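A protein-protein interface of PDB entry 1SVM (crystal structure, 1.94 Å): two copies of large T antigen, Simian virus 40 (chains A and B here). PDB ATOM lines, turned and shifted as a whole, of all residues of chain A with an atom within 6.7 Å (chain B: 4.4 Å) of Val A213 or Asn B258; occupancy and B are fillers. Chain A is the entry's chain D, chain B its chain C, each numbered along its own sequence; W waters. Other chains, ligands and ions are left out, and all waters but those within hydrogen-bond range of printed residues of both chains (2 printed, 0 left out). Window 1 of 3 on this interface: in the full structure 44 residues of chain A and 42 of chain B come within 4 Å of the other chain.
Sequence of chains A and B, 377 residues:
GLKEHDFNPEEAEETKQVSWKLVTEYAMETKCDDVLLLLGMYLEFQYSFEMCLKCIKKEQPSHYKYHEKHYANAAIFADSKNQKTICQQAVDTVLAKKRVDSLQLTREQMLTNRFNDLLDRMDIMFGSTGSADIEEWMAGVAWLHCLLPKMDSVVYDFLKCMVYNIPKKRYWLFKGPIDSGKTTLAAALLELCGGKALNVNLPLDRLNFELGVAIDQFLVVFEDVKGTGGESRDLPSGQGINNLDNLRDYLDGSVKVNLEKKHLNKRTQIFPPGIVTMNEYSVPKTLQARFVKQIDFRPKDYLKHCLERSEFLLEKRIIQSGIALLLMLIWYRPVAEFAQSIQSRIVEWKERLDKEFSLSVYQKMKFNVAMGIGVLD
Of chain B, only Asn B258 and Asn B265 come within 4 Å of Val A213.
Of the printed residues of chain A, Asn B258 touches Ala A197, Leu A198, Glu A210 and Val A213.
Of the printed residues of chain A, Thr B268 touches Lys A196.
Of the printed residues of chain A, Asn B265 touches Phe A209 (3.2 Å) and Val A213 (3.7 Å).
Of the printed residues of chain B, Ala A197 touches Asn B258.
Of the printed residues of chain A, Glu B260 touches Phe A209 (3.2 Å).
Of the printed residues of chain A, Tyr B250 touches Asn A199.
The nearest residue of chain A that does not touch Asn B258 is Lys A196 (4.1 Å).
The nearest printed residue of chain B that does not touch Leu A198 is Val B257 (7.2 Å).
Of the 19 printed residues of chain A, 7 touch a printed residue of chain B.
Hydrophobic or aromatic side chains of chain A within 4 Å of the printed part of chain B: Leu A198, Phe A209 and Val A213.
Along chain A the printed residues that touch a printed residue of chain B span positions 196 to 213.
Among the printed residues, 9 pairs touch across the chains.
Among the printed residues, no Asp or Glu carboxylate lies within 4 Å of a Lys or Arg side-chain nitrogen of the other chain.
Water W2 lies within hydrogen-bond range of N of Ala A197 and OD1 of Asn B258.
Water W1 lies within hydrogen-bond range of N of Asn B258 (3.0 Å), OE2 of Glu A210 (3.0 Å) and OH of Tyr B250 (3.1 Å).
Among the printed residues, pairs that only touch across the chains: Phe A209 with Glu B260 (3.2 Å), Phe A209 with Asn B265 (3.2 Å), Val A213 with Asn B265 (3.7 Å), Val A213 with Asn B258 (3.7 Å), Asn A199 with Tyr B250 (3.9 Å), Leu A198 with Asn B258 (3.9 Å) and Lys A196 with Thr B268 (3.9 Å).
OG1 of Thr B268 is in hydrogen-bond range of OD1 of Asn B258, 3.1 Å away.
O of Leu B259 sits close to OD1 of Asn B265 (3.1 Å).
The side-chain amino group of Lys A196 sits close to the side-chain amide nitrogen of Gln A217 (3.0 Å).
The side-chain carboxylate of Glu A210 is in hydrogen-bond range of the backbone NH of Asn A199 (2.9 Å).
2 positions are printed for both chains.
The side-chain amide nitrogen of Asn B258 lies within hydrogen-bond range of the backbone carbonyl oxygen of Ala A197, 3.0 Å away.
The side-chain carboxylate (OE2) of Glu A210 is in hydrogen-bond range of the side-chain amide nitrogen (ND2) of Asn B258.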
ATOM      1  N   GLY A 195     -17.754   0.041 -28.211  1.00  0.00           N
ATOM      2  CA  GLY A 195     -18.554   0.499 -27.092  1.00  0.00           C
ATOM      3  C   GLY A 195     -20.001   0.121 -27.320  1.00  0.00           C
ATOM      4  O   GLY A 195     -20.282  -0.776 -28.111  1.00  0.00           O
ATOM      5  N   LYS A 196     -20.921   0.811 -26.651  1.00  0.00           N
ATOM      6  CA  LYS A 196     -22.343   0.518 -26.787  1.00  0.00           C
ATOM      7  C   LYS A 196     -23.194   1.783 -26.886  1.00  0.00           C
ATOM      8  O   LYS A 196     -22.805   2.847 -26.398  1.00  0.00           O
ATOM      9  CB  LYS A 196     -22.824  -0.302 -25.578  1.00  0.00           C
ATOM     10  CG  LYS A 196     -22.192  -1.686 -25.469  1.00  0.00           C
ATOM     11  CD  LYS A 196     -22.739  -2.615 -26.541  1.00  0.00           C
ATOM     12  CE  LYS A 196     -21.960  -3.914 -26.610  1.00  0.00           C
ATOM     13  NZ  LYS A 196     -20.564  -3.678 -27.096  1.00  0.00           N
ATOM     14  N   ALA A 197     -24.353   1.655 -27.525  1.00  0.00           N
ATOM     15  CA  ALA A 197     -25.295   2.766 -27.653  1.00  0.00           C
ATOM     16  C   ALA A 197     -26.386   2.453 -26.635  1.00  0.00           C
ATOM     17  O   ALA A 197     -26.912   1.341 -26.602  1.00  0.00           O
ATOM     18  CB  ALA A 197     -25.887   2.817 -29.070  1.00  0.00           C
ATOM     19  N   LEU A 198     -26.728   3.423 -25.799  1.00  0.00           N
ATOM     20  CA  LEU A 198     -27.737   3.195 -24.771  1.00  0.00           C
ATOM     21  C   LEU A 198     -28.958   4.071 -24.990  1.00  0.00           C
ATOM     22  O   LEU A 198     -28.838   5.213 -25.435  1.00  0.00           O
ATOM     23  CB  LEU A 198     -27.150   3.492 -23.384  1.00  0.00           C
ATOM     24  CG  LEU A 198     -25.792   2.875 -23.045  1.00  0.00           C
ATOM     25  CD1 LEU A 198     -25.362   3.315 -21.651  1.00  0.00           C
ATOM     26  CD2 LEU A 198     -25.874   1.364 -23.125  1.00  0.00           C
ATOM     27  N   ASN A 199     -30.126   3.535 -24.656  1.00  0.00           N
ATOM     28  CA  ASN A 199     -31.379   4.267 -24.802  1.00  0.00           C
ATOM     29  C   ASN A 199     -31.916   4.641 -23.424  1.00  0.00           C
ATOM     30  O   ASN A 199     -32.360   3.772 -22.682  1.00  0.00           O
ATOM     31  CB  ASN A 199     -32.416   3.403 -25.523  1.00  0.00           C
ATOM     32  CG  ASN A 199     -33.683   4.174 -25.861  1.00  0.00           C
ATOM     33  OD1 ASN A 199     -34.175   4.966 -25.051  1.00  0.00           O
ATOM     34  ND2 ASN A 199     -34.221   3.941 -27.056  1.00  0.00           N
ATOM     35  N   ASN A 208     -31.673   0.865 -15.106  1.00  0.00           N
ATOM     36  CA  ASN A 208     -30.489   0.244 -14.523  1.00  0.00           C
ATOM     37  C   ASN A 208     -29.906  -0.831 -15.434  1.00  0.00           C
ATOM     38  O   ASN A 208     -28.697  -0.878 -15.649  1.00  0.00           O
ATOM     39  CB  ASN A 208     -30.819  -0.377 -13.160  1.00  0.00           C
ATOM     40  CG  ASN A 208     -31.109   0.666 -12.095  1.00  0.00           C
ATOM     41  OD1 ASN A 208     -32.043   1.456 -12.219  1.00  0.00           O
ATOM     42  ND2 ASN A 208     -30.303   0.670 -11.039  1.00  0.00           N
ATOM     43  N   PHE A 209     -30.767  -1.688 -15.972  1.00  0.00           N
ATOM     44  CA  PHE A 209     -30.301  -2.763 -16.838  1.00  0.00           C
ATOM     45  C   PHE A 209     -29.727  -2.234 -18.148  1.00  0.00           C
ATOM     46  O   PHE A 209     -28.800  -2.821 -18.700  1.00  0.00           O
ATOM     47  CB  PHE A 209     -31.430  -3.755 -17.125  1.00  0.00           C
ATOM     48  CG  PHE A 209     -30.947  -5.158 -17.368  1.00  0.00           C
ATOM     49  CD1 PHE A 209     -30.304  -5.868 -16.356  1.00  0.00           C
ATOM     50  CD2 PHE A 209     -31.113  -5.766 -18.610  1.00  0.00           C
ATOM     51  CE1 PHE A 209     -29.831  -7.163 -16.575  1.00  0.00           C
ATOM     52  CE2 PHE A 209     -30.644  -7.062 -18.841  1.00  0.00           C
ATOM     53  CZ  PHE A 209     -30.002  -7.760 -17.820  1.00  0.00           C
ATOM     54  N   GLU A 210     -30.283  -1.134 -18.649  1.00  0.00           N
ATOM     55  CA  GLU A 210     -29.780  -0.540 -19.884  1.00  0.00           C
ATOM     56  C   GLU A 210     -28.387   0.008 -19.583  1.00  0.00           C
ATOM     57  O   GLU A 210     -27.456  -0.169 -20.366  1.00  0.00           O
ATOM     58  CB  GLU A 210     -30.704   0.588 -20.357  1.00  0.00           C
ATOM     59  CG  GLU A 210     -30.292   1.259 -21.682  1.00  0.00           C
ATOM     60  CD  GLU A 210     -30.370   0.332 -22.896  1.00  0.00           C
ATOM     61  OE1 GLU A 210     -30.905  -0.790 -22.773  1.00  0.00           O
ATOM     62  OE2 GLU A 210     -29.903   0.731 -23.985  1.00  0.00           O
ATOM     63  N   LEU A 211     -28.239   0.653 -18.429  1.00  0.00           N
ATOM     64  CA  LEU A 211     -26.949   1.204 -18.046  1.00  0.00           C
ATOM     65  C   LEU A 211     -25.942   0.076 -17.807  1.00  0.00           C
ATOM     66  O   LEU A 211     -24.741   0.260 -17.997  1.00  0.00           O
ATOM     67  CB  LEU A 211     -27.087   2.073 -16.790  1.00  0.00           C
ATOM     68  CG  LEU A 211     -27.845   3.398 -16.958  1.00  0.00           C
ATOM     69  CD1 LEU A 211     -28.043   4.061 -15.602  1.00  0.00           C
ATOM     70  CD2 LEU A 211     -27.066   4.315 -17.884  1.00  0.00           C
ATOM     71  N   GLY A 212     -26.441  -1.095 -17.412  1.00  0.00           N
ATOM     72  CA  GLY A 212     -25.565  -2.232 -17.176  1.00  0.00           C
ATOM     73  C   GLY A 212     -24.813  -2.694 -18.420  1.00  0.00           C
ATOM     74  O   GLY A 212     -23.781  -3.357 -18.322  1.00  0.00           O
ATOM     75  N   VAL A 213     -25.334  -2.355 -19.596  1.00  0.00           N
ATOM     76  CA  VAL A 213     -24.695  -2.731 -20.859  1.00  0.00           C
ATOM     77  C   VAL A 213     -23.320  -2.057 -21.015  1.00  0.00           C
ATOM     78  O   VAL A 213     -22.461  -2.545 -21.743  1.00  0.00           O
ATOM     79  CB  VAL A 213     -25.607  -2.345 -22.065  1.00  0.00           C
ATOM     80  CG1 VAL A 213     -24.886  -2.573 -23.391  1.00  0.00           C
ATOM     81  CG2 VAL A 213     -26.879  -3.172 -22.030  1.00  0.00           C
ATOM     82  N   ALA A 214     -23.111  -0.944 -20.317  1.00  0.00           N
ATOM     83  CA  ALA A 214     -21.851  -0.211 -20.404  1.00  0.00           C
ATOM     84  C   ALA A 214     -20.679  -0.868 -19.683  1.00  0.00           C
ATOM     85  O   ALA A 214     -19.543  -0.427 -19.833  1.00  0.00           O
ATOM     86  CB  ALA A 214     -22.032   1.212 -19.875  1.00  0.00           C
ATOM     87  N   ILE A 215     -20.949  -1.911 -18.905  1.00  0.00           N
ATOM     88  CA  ILE A 215     -19.882  -2.586 -18.180  1.00  0.00           C
ATOM     89  C   ILE A 215     -18.733  -2.985 -19.105  1.00  0.00           C
ATOM     90  O   ILE A 215     -18.942  -3.599 -20.149  1.00  0.00           O
ATOM     91  CB  ILE A 215     -20.422  -3.830 -17.432  1.00  0.00           C
ATOM     92  CG1 ILE A 215     -21.314  -3.370 -16.271  1.00  0.00           C
ATOM     93  CG2 ILE A 215     -19.270  -4.674 -16.888  1.00  0.00           C
ATOM     94  CD1 ILE A 215     -22.073  -4.492 -15.577  1.00  0.00           C
ATOM     95  N   ASP A 216     -17.521  -2.610 -18.705  1.00  0.00           N
ATOM     96  CA  ASP A 216     -16.298  -2.909 -19.448  1.00  0.00           C
ATOM     97  C   ASP A 216     -16.223  -2.325 -20.865  1.00  0.00           C
ATOM     98  O   ASP A 216     -15.379  -2.750 -21.657  1.00  0.00           O
ATOM     99  CB  ASP A 216     -16.065  -4.432 -19.518  1.00  0.00           C
ATOM    100  CG  ASP A 216     -15.794  -5.065 -18.140  1.00  0.00           C
ATOM    101  OD1 ASP A 216     -15.238  -4.388 -17.254  1.00  0.00           O
ATOM    102  OD2 ASP A 216     -16.123  -6.257 -17.953  1.00  0.00           O
ATOM    103  N   GLN A 217     -17.085  -1.358 -21.187  1.00  0.00           N
ATOM    104  CA  GLN A 217     -17.072  -0.748 -22.526  1.00  0.00           C
ATOM    105  C   GLN A 217     -16.132   0.452 -22.590  1.00  0.00           C
ATOM    106  O   GLN A 217     -15.991   1.182 -21.613  1.00  0.00           O
ATOM    107  CB  GLN A 217     -18.484  -0.305 -22.923  1.00  0.00           C
ATOM    108  CG  GLN A 217     -19.491  -1.435 -22.899  1.00  0.00           C
ATOM    109  CD  GLN A 217     -19.093  -2.565 -23.821  1.00  0.00           C
ATOM    110  OE1 GLN A 217     -19.043  -3.725 -23.417  1.00  0.00           O
ATOM    111  NE2 GLN A 217     -18.809  -2.232 -25.069  1.00  0.00           N
ATOM    112  N   VAL A 220     -19.540   5.107 -24.495  1.00  0.00           N
ATOM    113  CA  VAL A 220     -20.979   4.953 -24.631  1.00  0.00           C
ATOM    114  C   VAL A 220     -21.612   6.118 -25.387  1.00  0.00           C
ATOM    115  O   VAL A 220     -21.151   7.253 -25.297  1.00  0.00           O
ATOM    116  CB  VAL A 220     -21.628   4.834 -23.225  1.00  0.00           C
ATOM    117  CG1 VAL A 220     -23.107   5.179 -23.285  1.00  0.00           C
ATOM    118  CG2 VAL A 220     -21.441   3.415 -22.695  1.00  0.00           C
ATOM    119  N   LEU A 259     -22.883  -0.707 -11.567  1.00  0.00           N
ATOM    120  CA  LEU A 259     -23.588  -1.259 -12.715  1.00  0.00           C
ATOM    121  C   LEU A 259     -24.006  -2.709 -12.504  1.00  0.00           C
ATOM    122  O   LEU A 259     -23.259  -3.498 -11.930  1.00  0.00           O
ATOM    123  CB  LEU A 259     -22.688  -1.158 -13.953  1.00  0.00           C
ATOM    124  CG  LEU A 259     -22.633   0.136 -14.783  1.00  0.00           C
ATOM    125  CD1 LEU A 259     -22.960   1.347 -13.956  1.00  0.00           C
ATOM    126  CD2 LEU A 259     -21.265   0.259 -15.427  1.00  0.00           C
ATOM    127  N   GLU A 260     -25.199  -3.052 -12.982  1.00  0.00           N
ATOM    128  CA  GLU A 260     -25.709  -4.412 -12.860  1.00  0.00           C
ATOM    129  C   GLU A 260     -26.099  -4.957 -14.233  1.00  0.00           C
ATOM    130  O   GLU A 260     -26.920  -4.368 -14.934  1.00  0.00           O
ATOM    131  CB  GLU A 260     -26.921  -4.449 -11.921  1.00  0.00           C
ATOM    132  CG  GLU A 260     -28.162  -3.737 -12.445  1.00  0.00           C
ATOM    133  CD  GLU A 260     -29.368  -3.920 -11.533  1.00  0.00           C
ATOM    134  OE1 GLU A 260     -29.675  -5.079 -11.177  1.00  0.00           O
ATOM    135  OE2 GLU A 260     -30.011  -2.908 -11.176  1.00  0.00           O
ATOM    136  N   LYS A 261     -25.498  -6.080 -14.614  1.00  0.00           N
ATOM    137  CA  LYS A 261     -25.783  -6.702 -15.903  1.00  0.00           C
ATOM    138  C   LYS A 261     -25.835  -8.221 -15.775  1.00  0.00           C
ATOM    139  O   LYS A 261     -24.901  -8.924 -16.163  1.00  0.00           O
ATOM    140  CB  LYS A 261     -24.719  -6.299 -16.933  1.00  0.00           C
ATOM    141  CG  LYS A 261     -24.925  -6.896 -18.320  1.00  0.00           C
ATOM    142  CD  LYS A 261     -23.973  -6.289 -19.346  1.00  0.00           C
ATOM    143  CE  LYS A 261     -22.518  -6.510 -18.970  1.00  0.00           C
ATOM    144  NZ  LYS A 261     -22.187  -7.955 -18.854  1.00  0.00           N
ATOM    145  N   TYR B 250     -34.020   2.275 -32.634  1.00  0.00           N
ATOM    146  CA  TYR B 250     -34.455   0.953 -33.056  1.00  0.00           C
ATOM    147  C   TYR B 250     -34.903   1.059 -34.518  1.00  0.00           C
ATOM    148  O   TYR B 250     -34.503   0.258 -35.360  1.00  0.00           O
ATOM    149  CB  TYR B 250     -35.625   0.460 -32.196  1.00  0.00           C
ATOM    150  CG  TYR B 250     -35.250   0.001 -30.797  1.00  0.00           C
ATOM    151  CD1 TYR B 250     -34.584   0.848 -29.916  1.00  0.00           C
ATOM    152  CD2 TYR B 250     -35.575  -1.286 -30.358  1.00  0.00           C
ATOM    153  CE1 TYR B 250     -34.243   0.424 -28.623  1.00  0.00           C
ATOM    154  CE2 TYR B 250     -35.245  -1.720 -29.074  1.00  0.00           C
ATOM    155  CZ  TYR B 250     -34.577  -0.861 -28.213  1.00  0.00           C
ATOM    156  OH  TYR B 250     -34.218  -1.293 -26.954  1.00  0.00           O
ATOM    157  N   VAL B 257     -28.735  -1.967 -31.072  1.00  0.00           N
ATOM    158  CA  VAL B 257     -29.575  -1.783 -29.897  1.00  0.00           C
ATOM    159  C   VAL B 257     -29.376  -2.971 -28.951  1.00  0.00           C
ATOM    160  O   VAL B 257     -28.843  -4.007 -29.352  1.00  0.00           O
ATOM    161  CB  VAL B 257     -31.055  -1.644 -30.331  1.00  0.00           C
ATOM    162  CG1 VAL B 257     -31.973  -2.078 -29.226  1.00  0.00           C
ATOM    163  CG2 VAL B 257     -31.339  -0.188 -30.717  1.00  0.00           C
ATOM    164  N   ASN B 258     -29.797  -2.828 -27.697  1.00  0.00           N
ATOM    165  CA  ASN B 258     -29.600  -3.895 -26.716  1.00  0.00           C
ATOM    166  C   ASN B 258     -30.907  -4.596 -26.380  1.00  0.00           C
ATOM    167  O   ASN B 258     -31.716  -4.086 -25.607  1.00  0.00           O
ATOM    168  CB  ASN B 258     -28.952  -3.305 -25.459  1.00  0.00           C
ATOM    169  CG  ASN B 258     -27.844  -2.315 -25.793  1.00  0.00           C
ATOM    170  OD1 ASN B 258     -26.887  -2.652 -26.495  1.00  0.00           O
ATOM    171  ND2 ASN B 258     -27.973  -1.088 -25.297  1.00  0.00           N
ATOM    172  N   LEU B 259     -31.103  -5.769 -26.974  1.00  0.00           N
ATOM    173  CA  LEU B 259     -32.327  -6.544 -26.781  1.00  0.00           C
ATOM    174  C   LEU B 259     -32.212  -7.584 -25.672  1.00  0.00           C
ATOM    175  O   LEU B 259     -31.276  -8.389 -25.644  1.00  0.00           O
ATOM    176  CB  LEU B 259     -32.720  -7.213 -28.099  1.00  0.00           C
ATOM    177  CG  LEU B 259     -32.876  -6.237 -29.276  1.00  0.00           C
ATOM    178  CD1 LEU B 259     -33.235  -7.008 -30.533  1.00  0.00           C
ATOM    179  CD2 LEU B 259     -33.952  -5.195 -28.956  1.00  0.00           C
ATOM    180  N   GLU B 260     -33.188  -7.558 -24.768  1.00  0.00           N
ATOM    181  CA  GLU B 260     -33.229  -8.452 -23.617  1.00  0.00           C
ATOM    182  C   GLU B 260     -34.079  -9.701 -23.833  1.00  0.00           C
ATOM    183  O   GLU B 260     -35.121  -9.659 -24.483  1.00  0.00           O
ATOM    184  CB  GLU B 260     -33.747  -7.679 -22.401  1.00  0.00           C
ATOM    185  CG  GLU B 260     -33.882  -8.498 -21.131  1.00  0.00           C
ATOM    186  CD  GLU B 260     -34.537  -7.714 -20.010  1.00  0.00           C
ATOM    187  OE1 GLU B 260     -33.965  -6.689 -19.585  1.00  0.00           O
ATOM    188  OE2 GLU B 260     -35.629  -8.124 -19.560  1.00  0.00           O
ATOM    189  N   ASN B 265     -29.899  -9.437 -20.858  1.00  0.00           N
ATOM    190  CA  ASN B 265     -29.660  -8.912 -22.196  1.00  0.00           C
ATOM    191  C   ASN B 265     -28.935 -10.001 -22.980  1.00  0.00           C
ATOM    192  O   ASN B 265     -27.795 -10.346 -22.666  1.00  0.00           O
ATOM    193  CB  ASN B 265     -28.800  -7.647 -22.127  1.00  0.00           C
ATOM    194  CG  ASN B 265     -28.943  -6.777 -23.363  1.00  0.00           C
ATOM    195  OD1 ASN B 265     -28.628  -7.198 -24.478  1.00  0.00           O
ATOM    196  ND2 ASN B 265     -29.425  -5.554 -23.170  1.00  0.00           N
ATOM    197  N   ARG B 267     -28.719 -10.001 -26.621  1.00  0.00           N
ATOM    198  CA  ARG B 267     -28.173  -9.611 -27.917  1.00  0.00           C
ATOM    199  C   ARG B 267     -28.134  -8.126 -28.264  1.00  0.00           C
ATOM    200  O   ARG B 267     -29.134  -7.413 -28.144  1.00  0.00           O
ATOM    201  CB  ARG B 267     -28.924 -10.336 -29.036  1.00  0.00           C
ATOM    202  CG  ARG B 267     -28.022 -10.876 -30.127  1.00  0.00           C
ATOM    203  CD  ARG B 267     -27.548 -12.276 -29.767  1.00  0.00           C
ATOM    204  NE  ARG B 267     -28.631 -13.252 -29.892  1.00  0.00           N
ATOM    205  CZ  ARG B 267     -28.538 -14.530 -29.541  1.00  0.00           C
ATOM    206  NH1 ARG B 267     -27.409 -15.002 -29.033  1.00  0.00           N
ATOM    207  NH2 ARG B 267     -29.574 -15.340 -29.712  1.00  0.00           N
ATOM    208  N   THR B 268     -26.963  -7.671 -28.701  1.00  0.00           N
ATOM    209  CA  THR B 268     -26.787  -6.297 -29.146  1.00  0.00           C
ATOM    210  C   THR B 268     -26.774  -6.444 -30.663  1.00  0.00           C
ATOM    211  O   THR B 268     -25.905  -7.114 -31.226  1.00  0.00           O
ATOM    212  CB  THR B 268     -25.450  -5.683 -28.646  1.00  0.00           C
ATOM    213  OG1 THR B 268     -25.556  -5.382 -27.247  1.00  0.00           O
ATOM    214  CG2 THR B 268     -25.131  -4.394 -29.398  1.00  0.00           C
HETATM  215  O   HOH W   1     -31.222  -0.542 -26.393  1.00  0.00           O
HETATM  216  O   HOH W   2     -25.336  -0.983 -28.354  1.00  0.00           O
